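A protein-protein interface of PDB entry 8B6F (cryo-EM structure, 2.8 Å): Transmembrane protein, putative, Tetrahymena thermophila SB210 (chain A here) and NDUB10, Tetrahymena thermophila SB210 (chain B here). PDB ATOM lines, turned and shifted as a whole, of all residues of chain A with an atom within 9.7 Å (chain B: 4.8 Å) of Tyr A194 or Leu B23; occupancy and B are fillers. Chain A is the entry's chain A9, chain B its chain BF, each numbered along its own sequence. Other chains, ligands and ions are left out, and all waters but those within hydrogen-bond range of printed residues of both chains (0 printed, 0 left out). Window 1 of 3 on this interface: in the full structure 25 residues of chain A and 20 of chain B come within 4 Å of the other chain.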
ATOM      1  N   ASP A  10      22.166  -8.450  36.099  1.00  0.00           N
ATOM      2  CA  ASP A  10      21.551  -8.189  34.801  1.00  0.00           C
ATOM      3  C   ASP A  10      20.065  -7.955  35.031  1.00  0.00           C
ATOM      4  O   ASP A  10      19.285  -8.902  35.140  1.00  0.00           O
ATOM      5  CB  ASP A  10      21.797  -9.347  33.842  1.00  0.00           C
ATOM      6  CG  ASP A  10      21.417  -9.009  32.416  1.00  0.00           C
ATOM      7  OD1 ASP A  10      20.854  -7.918  32.194  1.00  0.00           O
ATOM      8  OD2 ASP A  10      21.682  -9.831  31.514  1.00  0.00           O
ATOM      9  N   HIS A  12      17.745  -6.769  33.046  1.00  0.00           N
ATOM     10  CA  HIS A  12      16.902  -7.256  31.962  1.00  0.00           C
ATOM     11  C   HIS A  12      16.710  -8.765  32.042  1.00  0.00           C
ATOM     12  O   HIS A  12      15.589  -9.262  31.887  1.00  0.00           O
ATOM     13  CB  HIS A  12      17.506  -6.859  30.617  1.00  0.00           C
ATOM     14  CG  HIS A  12      16.771  -7.418  29.442  1.00  0.00           C
ATOM     15  ND1 HIS A  12      17.291  -8.418  28.648  1.00  0.00           N
ATOM     16  CD2 HIS A  12      15.553  -7.127  28.930  1.00  0.00           C
ATOM     17  CE1 HIS A  12      16.427  -8.712  27.696  1.00  0.00           C
ATOM     18  NE2 HIS A  12      15.362  -7.945  27.844  1.00  0.00           N
ATOM     19  N   TYR A  13      17.788  -9.509  32.287  1.00  0.00           N
ATOM     20  CA  TYR A  13      17.681 -10.963  32.334  1.00  0.00           C
ATOM     21  C   TYR A  13      16.831 -11.422  33.513  1.00  0.00           C
ATOM     22  O   TYR A  13      15.997 -12.323  33.369  1.00  0.00           O
ATOM     23  CB  TYR A  13      19.074 -11.584  32.396  1.00  0.00           C
ATOM     24  CG  TYR A  13      19.105 -13.025  31.954  1.00  0.00           C
ATOM     25  CD1 TYR A  13      18.859 -13.360  30.630  1.00  0.00           C
ATOM     26  CD2 TYR A  13      19.400 -14.045  32.846  1.00  0.00           C
ATOM     27  CE1 TYR A  13      18.890 -14.664  30.206  1.00  0.00           C
ATOM     28  CE2 TYR A  13      19.436 -15.362  32.428  1.00  0.00           C
ATOM     29  CZ  TYR A  13      19.179 -15.661  31.104  1.00  0.00           C
ATOM     30  OH  TYR A  13      19.208 -16.960  30.662  1.00  0.00           O
ATOM     31  N   VAL A  16      13.119 -10.681  32.668  1.00  0.00           N
ATOM     32  CA  VAL A  16      12.491 -11.595  31.719  1.00  0.00           C
ATOM     33  C   VAL A  16      12.270 -12.959  32.361  1.00  0.00           C
ATOM     34  O   VAL A  16      11.266 -13.630  32.094  1.00  0.00           O
ATOM     35  CB  VAL A  16      13.328 -11.704  30.431  1.00  0.00           C
ATOM     36  CG1 VAL A  16      13.404 -10.360  29.732  1.00  0.00           C
ATOM     37  CG2 VAL A  16      14.718 -12.220  30.737  1.00  0.00           C
ATOM     38  N   LEU A  17      13.201 -13.398  33.210  1.00  0.00           N
ATOM     39  CA  LEU A  17      13.041 -14.676  33.889  1.00  0.00           C
ATOM     40  C   LEU A  17      12.026 -14.624  35.023  1.00  0.00           C
ATOM     41  O   LEU A  17      11.507 -15.673  35.415  1.00  0.00           O
ATOM     42  CB  LEU A  17      14.380 -15.158  34.453  1.00  0.00           C
ATOM     43  CG  LEU A  17      15.463 -15.605  33.468  1.00  0.00           C
ATOM     44  CD1 LEU A  17      16.683 -16.073  34.238  1.00  0.00           C
ATOM     45  CD2 LEU A  17      14.973 -16.693  32.529  1.00  0.00           C
ATOM     46  N   GLU A 189      24.216 -16.441  34.835  1.00  0.00           N
ATOM     47  CA  GLU A 189      23.655 -16.627  33.508  1.00  0.00           C
ATOM     48  C   GLU A 189      24.410 -17.743  32.807  1.00  0.00           C
ATOM     49  O   GLU A 189      25.613 -17.921  33.012  1.00  0.00           O
ATOM     50  CB  GLU A 189      23.739 -15.348  32.669  1.00  0.00           C
ATOM     51  CG  GLU A 189      23.094 -14.141  33.318  1.00  0.00           C
ATOM     52  CD  GLU A 189      23.278 -12.880  32.500  1.00  0.00           C
ATOM     53  OE1 GLU A 189      24.049 -12.912  31.518  1.00  0.00           O
ATOM     54  OE2 GLU A 189      22.653 -11.856  32.837  1.00  0.00           O
ATOM     55  N   SER A 190      23.694 -18.491  31.975  1.00  0.00           N
ATOM     56  CA  SER A 190      24.317 -19.533  31.175  1.00  0.00           C
ATOM     57  C   SER A 190      25.059 -18.910  30.001  1.00  0.00           C
ATOM     58  O   SER A 190      24.578 -17.959  29.379  1.00  0.00           O
ATOM     59  CB  SER A 190      23.262 -20.519  30.674  1.00  0.00           C
ATOM     60  OG  SER A 190      23.845 -21.537  29.882  1.00  0.00           O
ATOM     61  N   ILE A 191      26.243 -19.447  29.702  1.00  0.00           N
ATOM     62  CA  ILE A 191      27.041 -18.919  28.604  1.00  0.00           C
ATOM     63  C   ILE A 191      26.321 -19.183  27.290  1.00  0.00           C
ATOM     64  O   ILE A 191      25.931 -20.319  26.992  1.00  0.00           O
ATOM     65  CB  ILE A 191      28.449 -19.538  28.611  1.00  0.00           C
ATOM     66  CG1 ILE A 191      29.319 -18.910  29.707  1.00  0.00           C
ATOM     67  CG2 ILE A 191      29.140 -19.365  27.260  1.00  0.00           C
ATOM     68  CD1 ILE A 191      28.895 -19.238  31.125  1.00  0.00           C
ATOM     69  N   GLY A 192      26.146 -18.132  26.495  1.00  0.00           N
ATOM     70  CA  GLY A 192      25.411 -18.222  25.255  1.00  0.00           C
ATOM     71  C   GLY A 192      23.925 -17.980  25.380  1.00  0.00           C
ATOM     72  O   GLY A 192      23.224 -18.005  24.361  1.00  0.00           O
ATOM     73  N   SER A 193      23.420 -17.742  26.587  1.00  0.00           N
ATOM     74  CA  SER A 193      21.998 -17.504  26.768  1.00  0.00           C
ATOM     75  C   SER A 193      21.596 -16.167  26.157  1.00  0.00           C
ATOM     76  O   SER A 193      22.413 -15.259  25.980  1.00  0.00           O
ATOM     77  CB  SER A 193      21.635 -17.530  28.252  1.00  0.00           C
ATOM     78  OG  SER A 193      22.347 -16.538  28.969  1.00  0.00           O
ATOM     79  N   TYR A 194      20.313 -16.053  25.831  1.00  0.00           N
ATOM     80  CA  TYR A 194      19.780 -14.850  25.210  1.00  0.00           C
ATOM     81  C   TYR A 194      18.280 -14.801  25.471  1.00  0.00           C
ATOM     82  O   TYR A 194      17.712 -15.685  26.117  1.00  0.00           O
ATOM     83  CB  TYR A 194      20.092 -14.821  23.712  1.00  0.00           C
ATOM     84  CG  TYR A 194      19.457 -15.950  22.934  1.00  0.00           C
ATOM     85  CD1 TYR A 194      18.185 -15.818  22.395  1.00  0.00           C
ATOM     86  CD2 TYR A 194      20.131 -17.146  22.736  1.00  0.00           C
ATOM     87  CE1 TYR A 194      17.600 -16.845  21.685  1.00  0.00           C
ATOM     88  CE2 TYR A 194      19.554 -18.180  22.026  1.00  0.00           C
ATOM     89  CZ  TYR A 194      18.289 -18.022  21.503  1.00  0.00           C
ATOM     90  OH  TYR A 194      17.708 -19.047  20.794  1.00  0.00           O
ATOM     91  N   THR A 195      17.645 -13.747  24.966  1.00  0.00           N
ATOM     92  CA  THR A 195      16.200 -13.592  25.026  1.00  0.00           C
ATOM     93  C   THR A 195      15.689 -13.237  23.639  1.00  0.00           C
ATOM     94  O   THR A 195      16.400 -12.627  22.838  1.00  0.00           O
ATOM     95  CB  THR A 195      15.773 -12.508  26.013  1.00  0.00           C
ATOM     96  OG1 THR A 195      16.231 -11.234  25.550  1.00  0.00           O
ATOM     97  CG2 THR A 195      16.360 -12.778  27.385  1.00  0.00           C
ATOM     98  N   THR A 196      14.452 -13.629  23.359  1.00  0.00           N
ATOM     99  CA  THR A 196      13.837 -13.428  22.054  1.00  0.00           C
ATOM    100  C   THR A 196      12.786 -12.332  22.150  1.00  0.00           C
ATOM    101  O   THR A 196      11.956 -12.340  23.063  1.00  0.00           O
ATOM    102  CB  THR A 196      13.194 -14.720  21.543  1.00  0.00           C
ATOM    103  OG1 THR A 196      12.112 -15.094  22.406  1.00  0.00           O
ATOM    104  CG2 THR A 196      14.216 -15.845  21.497  1.00  0.00           C
ATOM    105  N   PHE A 197      12.828 -11.394  21.206  1.00  0.00           N
ATOM    106  CA  PHE A 197      11.838 -10.334  21.106  1.00  0.00           C
ATOM    107  C   PHE A 197      11.356 -10.239  19.666  1.00  0.00           C
ATOM    108  O   PHE A 197      12.051 -10.634  18.729  1.00  0.00           O
ATOM    109  CB  PHE A 197      12.398  -8.981  21.564  1.00  0.00           C
ATOM    110  CG  PHE A 197      13.432  -8.404  20.639  1.00  0.00           C
ATOM    111  CD1 PHE A 197      14.773  -8.694  20.811  1.00  0.00           C
ATOM    112  CD2 PHE A 197      13.060  -7.560  19.606  1.00  0.00           C
ATOM    113  CE1 PHE A 197      15.724  -8.159  19.964  1.00  0.00           C
ATOM    114  CE2 PHE A 197      14.006  -7.023  18.757  1.00  0.00           C
ATOM    115  CZ  PHE A 197      15.339  -7.322  18.936  1.00  0.00           C
ATOM    116  N   LEU A 200       8.546 -13.210  15.544  1.00  0.00           N
ATOM    117  CA  LEU A 200       9.209 -14.067  14.571  1.00  0.00           C
ATOM    118  C   LEU A 200       8.700 -15.492  14.729  1.00  0.00           C
ATOM    119  O   LEU A 200       8.684 -16.032  15.839  1.00  0.00           O
ATOM    120  CB  LEU A 200      10.728 -14.035  14.746  1.00  0.00           C
ATOM    121  CG  LEU A 200      11.482 -12.760  14.363  1.00  0.00           C
ATOM    122  CD1 LEU A 200      12.970 -13.057  14.312  1.00  0.00           C
ATOM    123  CD2 LEU A 200      11.011 -12.180  13.038  1.00  0.00           C
ATOM    124  N   ARG A 205      12.957 -18.411  12.811  1.00  0.00           N
ATOM    125  CA  ARG A 205      14.065 -18.553  13.751  1.00  0.00           C
ATOM    126  C   ARG A 205      14.948 -19.738  13.379  1.00  0.00           C
ATOM    127  O   ARG A 205      16.178 -19.650  13.447  1.00  0.00           O
ATOM    128  CB  ARG A 205      13.531 -18.708  15.174  1.00  0.00           C
ATOM    129  CG  ARG A 205      12.579 -17.606  15.604  1.00  0.00           C
ATOM    130  CD  ARG A 205      12.607 -17.410  17.110  1.00  0.00           C
ATOM    131  NE  ARG A 205      13.795 -16.679  17.537  1.00  0.00           N
ATOM    132  CZ  ARG A 205      13.855 -15.364  17.701  1.00  0.00           C
ATOM    133  NH1 ARG A 205      12.799 -14.591  17.511  1.00  0.00           N
ATOM    134  NH2 ARG A 205      15.006 -14.809  18.065  1.00  0.00           N
ATOM    135  N   LYS A 206      14.337 -20.860  12.990  1.00  0.00           N
ATOM    136  CA  LYS A 206      15.121 -22.025  12.591  1.00  0.00           C
ATOM    137  C   LYS A 206      15.922 -21.744  11.328  1.00  0.00           C
ATOM    138  O   LYS A 206      17.073 -22.180  11.207  1.00  0.00           O
ATOM    139  CB  LYS A 206      14.210 -23.236  12.385  1.00  0.00           C
ATOM    140  CG  LYS A 206      13.662 -23.824  13.675  1.00  0.00           C
ATOM    141  CD  LYS A 206      13.025 -25.188  13.445  1.00  0.00           C
ATOM    142  CE  LYS A 206      11.853 -25.108  12.477  1.00  0.00           C
ATOM    143  NZ  LYS A 206      11.178 -26.426  12.308  1.00  0.00           N
ATOM    144  N   GLN A 208      17.077 -18.790  10.361  1.00  0.00           N
ATOM    145  CA  GLN A 208      18.194 -17.937  10.752  1.00  0.00           C
ATOM    146  C   GLN A 208      19.267 -18.735  11.480  1.00  0.00           C
ATOM    147  O   GLN A 208      20.465 -18.507  11.279  1.00  0.00           O
ATOM    148  CB  GLN A 208      17.699 -16.785  11.626  1.00  0.00           C
ATOM    149  CG  GLN A 208      18.790 -15.806  12.026  1.00  0.00           C
ATOM    150  CD  GLN A 208      19.531 -15.237  10.833  1.00  0.00           C
ATOM    151  OE1 GLN A 208      18.974 -15.111   9.745  1.00  0.00           O
ATOM    152  NE2 GLN A 208      20.800 -14.902  11.030  1.00  0.00           N
ATOM    153  N   GLU A 209      18.857 -19.682  12.326  1.00  0.00           N
ATOM    154  CA  GLU A 209      19.828 -20.515  13.027  1.00  0.00           C
ATOM    155  C   GLU A 209      20.576 -21.430  12.069  1.00  0.00           C
ATOM    156  O   GLU A 209      21.764 -21.700  12.279  1.00  0.00           O
ATOM    157  CB  GLU A 209      19.135 -21.328  14.119  1.00  0.00           C
ATOM    158  CG  GLU A 209      18.726 -20.494  15.324  1.00  0.00           C
ATOM    159  CD  GLU A 209      18.159 -21.327  16.455  1.00  0.00           C
ATOM    160  OE1 GLU A 209      18.029 -22.557  16.284  1.00  0.00           O
ATOM    161  OE2 GLU A 209      17.844 -20.753  17.518  1.00  0.00           O
ATOM    162  N   ASP A 212      23.149 -19.268  10.635  1.00  0.00           N
ATOM    163  CA  ASP A 212      24.197 -19.054  11.627  1.00  0.00           C
ATOM    164  C   ASP A 212      25.114 -20.263  11.723  1.00  0.00           C
ATOM    165  O   ASP A 212      26.333 -20.119  11.860  1.00  0.00           O
ATOM    166  CB  ASP A 212      23.581 -18.744  12.990  1.00  0.00           C
ATOM    167  CG  ASP A 212      22.930 -17.380  13.036  1.00  0.00           C
ATOM    168  OD1 ASP A 212      23.018 -16.644  12.032  1.00  0.00           O
ATOM    169  OD2 ASP A 212      22.331 -17.041  14.078  1.00  0.00           O
ATOM    170  N   SER B  12      27.545  -5.160  29.597  1.00  0.00           N
ATOM    171  CA  SER B  12      26.698  -4.461  28.647  1.00  0.00           C
ATOM    172  C   SER B  12      25.728  -5.429  27.974  1.00  0.00           C
ATOM    173  O   SER B  12      25.924  -6.646  27.967  1.00  0.00           O
ATOM    174  CB  SER B  12      27.545  -3.747  27.594  1.00  0.00           C
ATOM    175  OG  SER B  12      28.399  -4.653  26.922  1.00  0.00           O
ATOM    176  N   LEU B  13      24.669  -4.865  27.399  1.00  0.00           N
ATOM    177  CA  LEU B  13      23.657  -5.622  26.676  1.00  0.00           C
ATOM    178  C   LEU B  13      23.802  -5.380  25.181  1.00  0.00           C
ATOM    179  O   LEU B  13      24.017  -4.245  24.745  1.00  0.00           O
ATOM    180  CB  LEU B  13      22.247  -5.231  27.125  1.00  0.00           C
ATOM    181  CG  LEU B  13      21.836  -5.642  28.539  1.00  0.00           C
ATOM    182  CD1 LEU B  13      20.493  -5.030  28.898  1.00  0.00           C
ATOM    183  CD2 LEU B  13      21.779  -7.154  28.673  1.00  0.00           C
ATOM    184  N   ILE B  14      23.683  -6.451  24.402  1.00  0.00           N
ATOM    185  CA  ILE B  14      23.772  -6.396  22.948  1.00  0.00           C
ATOM    186  C   ILE B  14      22.401  -6.722  22.378  1.00  0.00           C
ATOM    187  O   ILE B  14      21.809  -7.753  22.718  1.00  0.00           O
ATOM    188  CB  ILE B  14      24.834  -7.369  22.410  1.00  0.00           C
ATOM    189  CG1 ILE B  14      26.208  -7.013  22.981  1.00  0.00           C
ATOM    190  CG2 ILE B  14      24.858  -7.338  20.881  1.00  0.00           C
ATOM    191  CD1 ILE B  14      27.305  -7.974  22.593  1.00  0.00           C
ATOM    192  N   ILE B  21      17.153 -10.852  18.878  1.00  0.00           N
ATOM    193  CA  ILE B  21      17.507 -11.411  20.177  1.00  0.00           C
ATOM    194  C   ILE B  21      18.295 -10.369  20.958  1.00  0.00           C
ATOM    195  O   ILE B  21      18.755  -9.365  20.414  1.00  0.00           O
ATOM    196  CB  ILE B  21      18.316 -12.723  20.064  1.00  0.00           C
ATOM    197  CG1 ILE B  21      19.629 -12.487  19.313  1.00  0.00           C
ATOM    198  CG2 ILE B  21      17.485 -13.793  19.380  1.00  0.00           C
ATOM    199  CD1 ILE B  21      20.527 -13.700  19.261  1.00  0.00           C
ATOM    200  N   ILE B  22      18.447 -10.624  22.256  1.00  0.00           N
ATOM    201  CA  ILE B  22      19.226  -9.776  23.149  1.00  0.00           C
ATOM    202  C   ILE B  22      20.202 -10.663  23.906  1.00  0.00           C
ATOM    203  O   ILE B  22      19.815 -11.718  24.420  1.00  0.00           O
ATOM    204  CB  ILE B  22      18.331  -8.995  24.131  1.00  0.00           C
ATOM    205  CG1 ILE B  22      17.256  -8.222  23.364  1.00  0.00           C
ATOM    206  CG2 ILE B  22      19.177  -8.049  24.976  1.00  0.00           C
ATOM    207  CD1 ILE B  22      16.264  -7.491  24.248  1.00  0.00           C
ATOM    208  N   LEU B  23      21.461 -10.242  23.968  1.00  0.00           N
ATOM    209  CA  LEU B  23      22.495 -10.970  24.683  1.00  0.00           C
ATOM    210  C   LEU B  23      23.181 -10.032  25.663  1.00  0.00           C
ATOM    211  O   LEU B  23      22.909  -8.830  25.708  1.00  0.00           O
ATOM    212  CB  LEU B  23      23.534 -11.569  23.725  1.00  0.00           C
ATOM    213  CG  LEU B  23      23.008 -12.459  22.599  1.00  0.00           C
ATOM    214  CD1 LEU B  23      22.563 -11.625  21.407  1.00  0.00           C
ATOM    215  CD2 LEU B  23      24.059 -13.470  22.185  1.00  0.00           C
ATOM    216  N   ASN B  24      24.080 -10.601  26.459  1.00  0.00           N
ATOM    217  CA  ASN B  24      24.913  -9.850  27.383  1.00  0.00           C
ATOM    218  C   ASN B  24      26.372 -10.106  27.041  1.00  0.00           C
ATOM    219  O   ASN B  24      26.741 -11.222  26.662  1.00  0.00           O
ATOM    220  CB  ASN B  24      24.621 -10.241  28.834  1.00  0.00           C
ATOM    221  CG  ASN B  24      25.198  -9.260  29.830  1.00  0.00           C
ATOM    222  OD1 ASN B  24      26.298  -8.746  29.645  1.00  0.00           O
ATOM    223  ND2 ASN B  24      24.450  -8.986  30.891  1.00  0.00           N
ATOM    224  N   THR B  25      27.201  -9.069  27.169  1.00  0.00           N
ATOM    225  CA  THR B  25      28.591  -9.180  26.739  1.00  0.00           C
ATOM    226  C   THR B  25      29.325 -10.269  27.508  1.00  0.00           C
ATOM    227  O   THR B  25      30.091 -11.044  26.923  1.00  0.00           O
ATOM    228  CB  THR B  25      29.301  -7.839  26.907  1.00  0.00           C
ATOM    229  OG1 THR B  25      28.599  -6.830  26.172  1.00  0.00           O
ATOM    230  CG2 THR B  25      30.734  -7.922  26.396  1.00  0.00           C
ATOM    231  N   LEU B  28      28.435 -14.048  26.298  1.00  0.00           N
ATOM    232  CA  LEU B  28      28.646 -14.521  24.938  1.00  0.00           C
ATOM    233  C   LEU B  28      29.579 -15.726  24.920  1.00  0.00           C
ATOM    234  O   LEU B  28      30.558 -15.785  25.668  1.00  0.00           O
ATOM    235  CB  LEU B  28      29.235 -13.408  24.075  1.00  0.00           C
ATOM    236  CG  LEU B  28      28.448 -12.102  24.001  1.00  0.00           C
ATOM    237  CD1 LEU B  28      29.166 -11.129  23.086  1.00  0.00           C
ATOM    238  CD2 LEU B  28      27.027 -12.344  23.522  1.00  0.00           C
ATOM    239  N   GLN B  32      29.156 -16.509  19.339  1.00  0.00           N
ATOM    240  CA  GLN B  32      28.474 -15.232  19.519  1.00  0.00           C
ATOM    241  C   GLN B  32      29.473 -14.087  19.585  1.00  0.00           C
ATOM    242  O   GLN B  32      29.224 -13.004  19.043  1.00  0.00           O
ATOM    243  CB  GLN B  32      27.605 -15.274  20.773  1.00  0.00           C
ATOM    244  CG  GLN B  32      26.437 -16.239  20.662  1.00  0.00           C
ATOM    245  CD  GLN B  32      25.648 -16.350  21.946  1.00  0.00           C
ATOM    246  OE1 GLN B  32      26.023 -15.782  22.967  1.00  0.00           O
ATOM    247  NE2 GLN B  32      24.544 -17.084  21.899  1.00  0.00           N
ATOM    248  N   TYR B  36      29.288 -10.943  16.938  1.00  0.00           N
ATOM    249  CA  TYR B  36      28.992  -9.586  17.390  1.00  0.00           C
ATOM    250  C   TYR B  36      30.268  -8.772  17.581  1.00  0.00           C
ATOM    251  O   TYR B  36      30.446  -7.729  16.945  1.00  0.00           O
ATOM    252  CB  TYR B  36      28.170  -9.650  18.681  1.00  0.00           C
ATOM    253  CG  TYR B  36      26.870 -10.396  18.487  1.00  0.00           C
ATOM    254  CD1 TYR B  36      26.041 -10.113  17.409  1.00  0.00           C
ATOM    255  CD2 TYR B  36      26.491 -11.406  19.357  1.00  0.00           C
ATOM    256  CE1 TYR B  36      24.865 -10.799  17.214  1.00  0.00           C
ATOM    257  CE2 TYR B  36      25.314 -12.098  19.171  1.00  0.00           C
ATOM    258  CZ  TYR B  36      24.506 -11.789  18.096  1.00  0.00           C
ATOM    259  OH  TYR B  36      23.336 -12.479  17.908  1.00  0.00           O
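O of Gly A192 lies within hydrogen-bond range of NE2 of Gln B32. The backbone carbonyl oxygen (O) of Thr A195 lies within hydrogen-bond range of the backbone NH (N) of Ile B22 (2.9 Å). OD2 of Asp A10 lies within hydrogen-bond range of ND2 of Asn B24 (3.0 Å).
The backbone carbonyl oxygen of Ser B12 sits close to the side-chain amide oxygen of Asn B24. The side-chain carboxylate (OD1) of Asp A10 sits at hydrogen-bond distance from the backbone NH (N) of Tyr A13 (3.5 Å). OE2 of Glu A189 lies close to OD2 of Asp A10 (2.6 Å). N of Leu B23 lies within hydrogen-bond range of O of Ile B14. The backbone NH (N) of His A12 sits close to the side-chain carboxylate (OD1) of Asp A10, at 3.4 Å.
Among the printed residues, merely in contact across the chains: Arg A205 with Ile B21 (3.0 Å), Thr A195 with Ile B21 (3.1 Å), Tyr A194 with Ile B22 (3.2 Å), Phe A197 with Ile B21 (3.2 Å), Phe A197 with Ile B22 (3.6 Å), His A12 with Ile B22 (3.7 Å), Tyr A194 with Ile B21 (3.7 Å), Asp A10 with Leu B13 (3.7 Å), Glu A189 with Asn B24 (3.8 Å), His A12 with Leu B13 (3.9 Å) and Tyr A194 with Leu B23 (3.9 Å).
Of the printed residues of chain B, Asp A10 touches Leu B13 (3.7 Å) and Asn B24 (3.0 Å). Tyr A13 touches none of the printed residues of chain B. Tyr A194 touches three residues of chain B. Of the printed residues of chain B, Arg A205 touches Ile B21 (3.0 Å). No residue of chain A comes within 4 Å of Ile B14. Leu B23 touches just one residue of chain A: Tyr A194. The nearest residue of chain A that does not touch Leu B23 is Ser A193 (4.4 Å).
Among the printed residues, no Asp or Glu carboxylate lies within 4 Å of a Lys or Arg side-chain nitrogen of the other chain.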
